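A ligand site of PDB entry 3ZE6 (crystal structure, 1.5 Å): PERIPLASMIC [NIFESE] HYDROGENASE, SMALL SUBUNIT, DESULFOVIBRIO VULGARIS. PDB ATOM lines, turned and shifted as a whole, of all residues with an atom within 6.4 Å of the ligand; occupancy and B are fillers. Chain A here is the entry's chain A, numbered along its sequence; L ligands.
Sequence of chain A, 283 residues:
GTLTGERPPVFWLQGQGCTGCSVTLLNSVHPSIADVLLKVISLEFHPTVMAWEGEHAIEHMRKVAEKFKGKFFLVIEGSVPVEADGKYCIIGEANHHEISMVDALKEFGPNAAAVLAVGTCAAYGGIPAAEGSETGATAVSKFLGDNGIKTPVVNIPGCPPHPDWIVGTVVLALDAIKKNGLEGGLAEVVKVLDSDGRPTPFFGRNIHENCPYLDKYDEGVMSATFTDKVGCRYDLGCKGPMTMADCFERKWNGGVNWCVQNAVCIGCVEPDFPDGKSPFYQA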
ATOM      1  N   ILE A 207      17.487  -5.321 -27.411  1.00  0.00           N
ATOM      2  CA  ILE A 207      16.222  -5.779 -26.856  1.00  0.00           C
ATOM      3  C   ILE A 207      16.230  -5.741 -25.335  1.00  0.00           C
ATOM      4  O   ILE A 207      15.339  -5.155 -24.718  1.00  0.00           O
ATOM      5  CB  ILE A 207      15.904  -7.204 -27.315  1.00  0.00           C
ATOM      6  CG1 ILE A 207      15.544  -7.191 -28.803  1.00  0.00           C
ATOM      7  CG2 ILE A 207      14.767  -7.792 -26.503  1.00  0.00           C
ATOM      8  CD1 ILE A 207      15.288  -8.544 -29.375  1.00  0.00           C
ATOM      9  N   HIS A 208      17.241  -6.348 -24.726  1.00  0.00           N
ATOM     10  CA  HIS A 208      17.307  -6.509 -23.285  1.00  0.00           C
ATOM     11  C   HIS A 208      17.321  -5.167 -22.533  1.00  0.00           C
ATOM     12  O   HIS A 208      16.620  -5.006 -21.517  1.00  0.00           O
ATOM     13  CB  HIS A 208      18.558  -7.345 -23.012  1.00  0.00           C
ATOM     14  CG  HIS A 208      18.925  -7.499 -21.573  1.00  0.00           C
ATOM     15  ND1 HIS A 208      18.264  -8.329 -20.706  1.00  0.00           N
ATOM     16  CD2 HIS A 208      19.944  -6.942 -20.860  1.00  0.00           C
ATOM     17  CE1 HIS A 208      18.840  -8.282 -19.518  1.00  0.00           C
ATOM     18  NE2 HIS A 208      19.863  -7.453 -19.589  1.00  0.00           N
ATOM     19  N   GLU A 209      18.056  -4.189 -23.055  1.00  0.00           N
ATOM     20  CA  GLU A 209      18.117  -2.866 -22.404  1.00  0.00           C
ATOM     21  C   GLU A 209      16.766  -2.182 -22.381  1.00  0.00           C
ATOM     22  O   GLU A 209      16.518  -1.316 -21.552  1.00  0.00           O
ATOM     23  CB  GLU A 209      19.152  -1.973 -23.086  1.00  0.00           C
ATOM     24  CG  GLU A 209      20.580  -2.480 -22.925  1.00  0.00           C
ATOM     25  CD  GLU A 209      21.595  -1.680 -23.745  1.00  0.00           C
ATOM     26  OE1 GLU A 209      21.212  -0.646 -24.345  1.00  0.00           O
ATOM     27  OE2 GLU A 209      22.760  -2.124 -23.805  1.00  0.00           O
ATOM     28  N   CYS A 211      13.775  -4.077 -22.420  1.00  0.00           N
ATOM     29  CA  CYS A 211      12.793  -5.122 -22.118  1.00  0.00           C
ATOM     30  C   CYS A 211      11.941  -4.797 -20.908  1.00  0.00           C
ATOM     31  O   CYS A 211      12.458  -4.365 -19.873  1.00  0.00           O
ATOM     32  CB  CYS A 211      13.500  -6.461 -21.887  1.00  0.00           C
ATOM     33  SG  CYS A 211      12.376  -7.835 -21.625  1.00  0.00           S
ATOM     34  N   PRO A 212      10.630  -5.074 -20.994  1.00  0.00           N
ATOM     35  CA  PRO A 212       9.771  -4.860 -19.832  1.00  0.00           C
ATOM     36  C   PRO A 212      10.072  -5.781 -18.631  1.00  0.00           C
ATOM     37  O   PRO A 212       9.520  -5.550 -17.552  1.00  0.00           O
ATOM     38  CB  PRO A 212       8.351  -5.118 -20.384  1.00  0.00           C
ATOM     39  CG  PRO A 212       8.571  -5.950 -21.593  1.00  0.00           C
ATOM     40  CD  PRO A 212       9.869  -5.561 -22.169  1.00  0.00           C
ATOM     41  N   TYR A 213      10.906  -6.807 -18.790  1.00  0.00           N
ATOM     42  CA  TYR A 213      11.252  -7.726 -17.700  1.00  0.00           C
ATOM     43  C   TYR A 213      12.642  -7.450 -17.137  1.00  0.00           C
ATOM     44  O   TYR A 213      13.139  -8.214 -16.316  1.00  0.00           O
ATOM     45  CB  TYR A 213      11.069  -9.204 -18.124  1.00  0.00           C
ATOM     46  CG  TYR A 213       9.709  -9.390 -18.799  1.00  0.00           C
ATOM     47  CD1 TYR A 213       8.522  -9.340 -18.073  1.00  0.00           C
ATOM     48  CD2 TYR A 213       9.637  -9.579 -20.155  1.00  0.00           C
ATOM     49  CE1 TYR A 213       7.291  -9.478 -18.734  1.00  0.00           C
ATOM     50  CE2 TYR A 213       8.446  -9.715 -20.798  1.00  0.00           C
ATOM     51  CZ  TYR A 213       7.288  -9.663 -20.103  1.00  0.00           C
ATOM     52  OH  TYR A 213       6.114  -9.809 -20.836  1.00  0.00           O
ATOM     53  N   LEU A 214      13.264  -6.357 -17.576  1.00  0.00           N
ATOM     54  CA  LEU A 214      14.636  -6.034 -17.143  1.00  0.00           C
ATOM     55  C   LEU A 214      14.665  -5.855 -15.625  1.00  0.00           C
ATOM     56  O   LEU A 214      15.646  -6.252 -14.977  1.00  0.00           O
ATOM     57  CB  LEU A 214      15.138  -4.780 -17.850  1.00  0.00           C
ATOM     58  CG  LEU A 214      16.601  -4.393 -17.551  1.00  0.00           C
ATOM     59  CD1 LEU A 214      17.592  -5.502 -17.915  1.00  0.00           C
ATOM     60  CD2 LEU A 214      16.930  -3.110 -18.281  1.00  0.00           C
ATOM     61  N   ASP A 215      13.604  -5.299 -15.051  1.00  0.00           N
ATOM     62  CA  ASP A 215      13.575  -5.184 -13.600  1.00  0.00           C
ATOM     63  C   ASP A 215      13.681  -6.563 -12.905  1.00  0.00           C
ATOM     64  O   ASP A 215      14.390  -6.721 -11.910  1.00  0.00           O
ATOM     65  CB  ASP A 215      12.374  -4.346 -13.104  1.00  0.00           C
ATOM     66  CG  ASP A 215      10.998  -4.930 -13.494  1.00  0.00           C
ATOM     67  OD1 ASP A 215      10.889  -5.768 -14.409  1.00  0.00           O
ATOM     68  OD2 ASP A 215       9.997  -4.520 -12.870  1.00  0.00           O
ATOM     69  N   LYS A 216      13.014  -7.569 -13.467  1.00  0.00           N
ATOM     70  CA  LYS A 216      13.072  -8.912 -12.921  1.00  0.00           C
ATOM     71  C   LYS A 216      14.463  -9.535 -13.107  1.00  0.00           C
ATOM     72  O   LYS A 216      14.997 -10.186 -12.218  1.00  0.00           O
ATOM     73  CB  LYS A 216      11.985  -9.782 -13.538  1.00  0.00           C
ATOM     74  CG  LYS A 216      10.579  -9.250 -13.320  1.00  0.00           C
ATOM     75  CD  LYS A 216      10.174  -9.377 -11.852  1.00  0.00           C
ATOM     76  CE  LYS A 216       8.789  -8.802 -11.575  1.00  0.00           C
ATOM     77  NZ  LYS A 216       8.414  -8.978 -10.147  1.00  0.00           N
ATOM     78  N   TYR A 217      15.057  -9.324 -14.273  1.00  0.00           N
ATOM     79  CA  TYR A 217      16.425  -9.738 -14.501  1.00  0.00           C
ATOM     80  C   TYR A 217      17.338  -9.183 -13.423  1.00  0.00           C
ATOM     81  O   TYR A 217      18.153  -9.912 -12.864  1.00  0.00           O
ATOM     82  CB  TYR A 217      16.872  -9.207 -15.867  1.00  0.00           C
ATOM     83  CG  TYR A 217      18.305  -9.480 -16.269  1.00  0.00           C
ATOM     84  CD1 TYR A 217      18.647 -10.659 -16.927  1.00  0.00           C
ATOM     85  CD2 TYR A 217      19.294  -8.539 -16.019  1.00  0.00           C
ATOM     86  CE1 TYR A 217      19.956 -10.879 -17.335  1.00  0.00           C
ATOM     87  CE2 TYR A 217      20.573  -8.750 -16.416  1.00  0.00           C
ATOM     88  CZ  TYR A 217      20.916  -9.919 -17.045  1.00  0.00           C
ATOM     89  OH  TYR A 217      22.224 -10.089 -17.414  1.00  0.00           O
ATOM     90  N   MET A 222      13.627 -15.191 -11.999  1.00  0.00           N
ATOM     91  CA  MET A 222      13.620 -15.946 -13.260  1.00  0.00           C
ATOM     92  C   MET A 222      12.481 -16.934 -13.303  1.00  0.00           C
ATOM     93  O   MET A 222      12.313 -17.745 -12.395  1.00  0.00           O
ATOM     94  CB  MET A 222      14.905 -16.775 -13.389  1.00  0.00           C
ATOM     95  CG  MET A 222      16.168 -15.953 -13.478  1.00  0.00           C
ATOM     96  SD  MET A 222      16.140 -14.888 -14.923  1.00  0.00           S
ATOM     97  CE  MET A 222      17.491 -13.735 -14.590  1.00  0.00           C
ATOM     98  N   GLY A 231       8.396 -13.663 -14.318  1.00  0.00           N
ATOM     99  CA  GLY A 231       9.851 -13.639 -14.235  1.00  0.00           C
ATOM    100  C   GLY A 231      10.531 -13.294 -15.547  1.00  0.00           C
ATOM    101  O   GLY A 231       9.930 -13.330 -16.624  1.00  0.00           O
ATOM    102  N   CYS A 232      11.799 -12.959 -15.450  1.00  0.00           N
ATOM    103  CA  CYS A 232      12.627 -12.825 -16.645  1.00  0.00           C
ATOM    104  C   CYS A 232      12.842 -14.222 -17.266  1.00  0.00           C
ATOM    105  O   CYS A 232      12.788 -15.269 -16.579  1.00  0.00           O
ATOM    106  CB  CYS A 232      13.956 -12.143 -16.255  1.00  0.00           C
ATOM    107  SG  CYS A 232      15.368 -12.355 -17.378  1.00  0.00           S
ATOM    108  N   ARG A 233      13.070 -14.213 -18.586  1.00  0.00           N
ATOM    109  CA  ARG A 233      13.167 -15.428 -19.394  1.00  0.00           C
ATOM    110  C   ARG A 233      14.627 -15.868 -19.625  1.00  0.00           C
ATOM    111  O   ARG A 233      14.901 -16.802 -20.384  1.00  0.00           O
ATOM    112  CB  ARG A 233      12.489 -15.192 -20.752  1.00  0.00           C
ATOM    113  CG  ARG A 233      10.952 -15.150 -20.763  1.00  0.00           C
ATOM    114  CD  ARG A 233      10.347 -13.915 -20.085  1.00  0.00           C
ATOM    115  NE  ARG A 233       8.994 -13.728 -20.576  1.00  0.00           N
ATOM    116  CZ  ARG A 233       7.980 -13.217 -19.893  1.00  0.00           C
ATOM    117  NH1 ARG A 233       8.099 -12.846 -18.631  1.00  0.00           N
ATOM    118  NH2 ARG A 233       6.817 -13.110 -20.490  1.00  0.00           N
ATOM    119  N   TYR A 234      15.580 -15.235 -18.950  1.00  0.00           N
ATOM    120  CA  TYR A 234      16.991 -15.527 -19.171  1.00  0.00           C
ATOM    121  C   TYR A 234      17.344 -16.997 -18.955  1.00  0.00           C
ATOM    122  O   TYR A 234      18.047 -17.597 -19.775  1.00  0.00           O
ATOM    123  CB  TYR A 234      17.867 -14.615 -18.276  1.00  0.00           C
ATOM    124  CG  TYR A 234      19.343 -14.892 -18.359  1.00  0.00           C
ATOM    125  CD1 TYR A 234      20.113 -14.318 -19.348  1.00  0.00           C
ATOM    126  CD2 TYR A 234      19.949 -15.759 -17.461  1.00  0.00           C
ATOM    127  CE1 TYR A 234      21.458 -14.582 -19.436  1.00  0.00           C
ATOM    128  CE2 TYR A 234      21.304 -16.023 -17.540  1.00  0.00           C
ATOM    129  CZ  TYR A 234      22.043 -15.430 -18.527  1.00  0.00           C
ATOM    130  OH  TYR A 234      23.409 -15.703 -18.606  1.00  0.00           O
ATOM    131  N   ASP A 235      16.880 -17.603 -17.878  1.00  0.00           N
ATOM    132  CA  ASP A 235      17.202 -19.003 -17.572  1.00  0.00           C
ATOM    133  C   ASP A 235      16.546 -19.964 -18.574  1.00  0.00           C
ATOM    134  O   ASP A 235      17.032 -21.070 -18.769  1.00  0.00           O
ATOM    135  CB  ASP A 235      16.749 -19.415 -16.178  1.00  0.00           C
ATOM    136  CG  ASP A 235      17.625 -18.891 -15.067  1.00  0.00           C
ATOM    137  OD1 ASP A 235      18.705 -18.322 -15.337  1.00  0.00           O
ATOM    138  OD2 ASP A 235      17.193 -19.104 -13.897  1.00  0.00           O
ATOM    139  N   CYS A 238      16.513 -16.920 -23.137  1.00  0.00           N
ATOM    140  CA  CYS A 238      16.333 -15.666 -23.837  1.00  0.00           C
ATOM    141  C   CYS A 238      17.655 -15.034 -24.247  1.00  0.00           C
ATOM    142  O   CYS A 238      18.548 -14.813 -23.394  1.00  0.00           O
ATOM    143  CB  CYS A 238      15.570 -14.668 -22.950  1.00  0.00           C
ATOM    144  SG  CYS A 238      15.139 -13.160 -23.804  1.00  0.00           S
ATOM    145  N   LYS A 239      17.775 -14.700 -25.537  1.00  0.00           N
ATOM    146  CA  LYS A 239      18.995 -14.125 -26.063  1.00  0.00           C
ATOM    147  C   LYS A 239      18.871 -12.612 -26.258  1.00  0.00           C
ATOM    148  O   LYS A 239      19.711 -12.000 -26.929  1.00  0.00           O
ATOM    149  CB  LYS A 239      19.423 -14.806 -27.371  1.00  0.00           C
ATOM    150  CG  LYS A 239      19.694 -16.302 -27.232  1.00  0.00           C
ATOM    151  CD  LYS A 239      20.633 -16.656 -26.053  1.00  0.00           C
ATOM    152  CE  LYS A 239      20.996 -18.128 -26.087  1.00  0.00           C
ATOM    153  NZ  LYS A 239      19.798 -18.999 -26.199  1.00  0.00           N
ATOM    154  N   GLY A 240      17.837 -12.004 -25.665  1.00  0.00           N
ATOM    155  CA  GLY A 240      17.672 -10.561 -25.728  1.00  0.00           C
ATOM    156  C   GLY A 240      18.953  -9.773 -25.408  1.00  0.00           C
ATOM    157  O   GLY A 240      19.212  -8.743 -26.002  1.00  0.00           O
ATOM    158  N   PRO A 241      19.729 -10.218 -24.411  1.00  0.00           N
ATOM    159  CA  PRO A 241      20.941  -9.444 -24.098  1.00  0.00           C
ATOM    160  C   PRO A 241      21.918  -9.270 -25.239  1.00  0.00           C
ATOM    161  O   PRO A 241      22.717  -8.323 -25.222  1.00  0.00           O
ATOM    162  CB  PRO A 241      21.583 -10.267 -22.981  1.00  0.00           C
ATOM    163  CG  PRO A 241      20.424 -10.917 -22.297  1.00  0.00           C
ATOM    164  CD  PRO A 241      19.508 -11.302 -23.447  1.00  0.00           C
ATOM    165  N   TRP A 258       4.836 -10.793 -28.981  1.00  0.00           N
ATOM    166  CA  TRP A 258       6.235 -10.858 -29.434  1.00  0.00           C
ATOM    167  C   TRP A 258       6.970 -11.980 -28.707  1.00  0.00           C
ATOM    168  O   TRP A 258       6.459 -12.570 -27.759  1.00  0.00           O
ATOM    169  CB  TRP A 258       6.946  -9.503 -29.280  1.00  0.00           C
ATOM    170  CG  TRP A 258       7.235  -9.031 -27.896  1.00  0.00           C
ATOM    171  CD1 TRP A 258       6.317  -8.772 -26.893  1.00  0.00           C
ATOM    172  CD2 TRP A 258       8.520  -8.690 -27.350  1.00  0.00           C
ATOM    173  NE1 TRP A 258       6.968  -8.311 -25.753  1.00  0.00           N
ATOM    174  CE2 TRP A 258       8.317  -8.247 -26.017  1.00  0.00           C
ATOM    175  CE3 TRP A 258       9.835  -8.721 -27.861  1.00  0.00           C
ATOM    176  CZ2 TRP A 258       9.378  -7.836 -25.192  1.00  0.00           C
ATOM    177  CZ3 TRP A 258      10.876  -8.301 -27.036  1.00  0.00           C
ATOM    178  CH2 TRP A 258      10.643  -7.879 -25.721  1.00  0.00           C
ATOM    179  N   VAL A 260       9.524 -12.472 -26.668  1.00  0.00           N
ATOM    180  CA  VAL A 260       9.881 -12.476 -25.251  1.00  0.00           C
ATOM    181  C   VAL A 260       8.631 -12.628 -24.380  1.00  0.00           C
ATOM    182  O   VAL A 260       8.652 -13.347 -23.370  1.00  0.00           O
ATOM    183  CB  VAL A 260      10.675 -11.204 -24.878  1.00  0.00           C
ATOM    184  CG1 VAL A 260      10.910 -11.124 -23.377  1.00  0.00           C
ATOM    185  CG2 VAL A 260      12.008 -11.176 -25.620  1.00  0.00           C
ATOM    186  N   CYS A 265      13.378 -14.736 -26.778  1.00  0.00           N
ATOM    187  CA  CYS A 265      14.065 -14.269 -27.981  1.00  0.00           C
ATOM    188  C   CYS A 265      15.170 -15.272 -28.361  1.00  0.00           C
ATOM    189  O   CYS A 265      15.892 -15.721 -27.473  1.00  0.00           O
ATOM    190  CB  CYS A 265      14.657 -12.870 -27.733  1.00  0.00           C
ATOM    191  SG  CYS A 265      15.711 -12.233 -29.073  1.00  0.00           S
HETATM  192 FE1  LIG L   1      15.191 -11.615 -22.055  1.00  0.00          FE
HETATM  193 FE2  LIG L   1      15.091 -11.140 -19.325  1.00  0.00          FE
HETATM  194 FE3  LIG L   1      13.990  -9.400 -21.097  1.00  0.00          FE
HETATM  195 FE4  LIG L   1      16.644  -9.586 -20.917  1.00  0.00          FE
HETATM  196  S1  LIG L   1      15.205  -8.869 -19.259  1.00  0.00           S
HETATM  197  S2  LIG L   1      15.470  -9.514 -22.874  1.00  0.00           S
HETATM  198  S3  LIG L   1      16.916 -11.830 -20.558  1.00  0.00           S
HETATM  199  S4  LIG L   1      13.307 -11.568 -20.702  1.00  0.00           S
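FE4 of the ligand is bound by ND1 of His 208. An iron atom (FE3) of the ligand is bound by the side-chain sulfur (SG) of Cys 211 (2.3 Å). An iron atom (FE2) of the ligand is bound by the side-chain sulfur of Cys 232 (2.3 Å). The side-chain sulfur (SG) of Cys 238 binds an iron atom (FE1) of the ligand. The backbone NH (N) of Arg 233 lies close to a sulfur (S4) of the ligand (3.4 Å). The backbone NH (N) of Leu 214 lies close to a sulfur (S1) of the ligand (3.6 Å).
The backbone carbonyl oxygen (O) of Gly 240 is in hydrogen-bond range of the backbone NH (N) of His 208 (3.4 Å). The side-chain sulfur (SG) of Cys 232 sits close to the backbone NH (N) of Tyr 234 (3.3 Å). The side-chain sulfur (SD) of Met 222 sits close to the side-chain sulfur (SG) of Cys 232 (3.6 Å). N of Cys 238 is in hydrogen-bond range of O of Arg 233, 3.2 Å away. The side-chain sulfur (SG) of Cys 238 lies close to the backbone NH (N) of Gly 240 (3.5 Å). The side-chain hydroxyl of Tyr 213 sits at hydrogen-bond distance from the guanidinium group of Arg 233. O of Val 260 is in hydrogen-bond range of NE of Arg 233 (2.8 Å). O of Gly 231 sits at hydrogen-bond distance from NH1 of Arg 233.
O of Tyr 213 sits close to S1 of the ligand, at 3.7 Å. Residues that only touch the ligand: Val 260, Tyr 234, Gly 240, Tyr 217 and Pro 241. Hydrophobic or aromatic side chains within 4 Å of the ligand: His 208, Tyr 217, Tyr 234, Pro 241 and Val 260. The nearest printed residue that does not touch the ligand is Ile 207 (4.1 Å).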
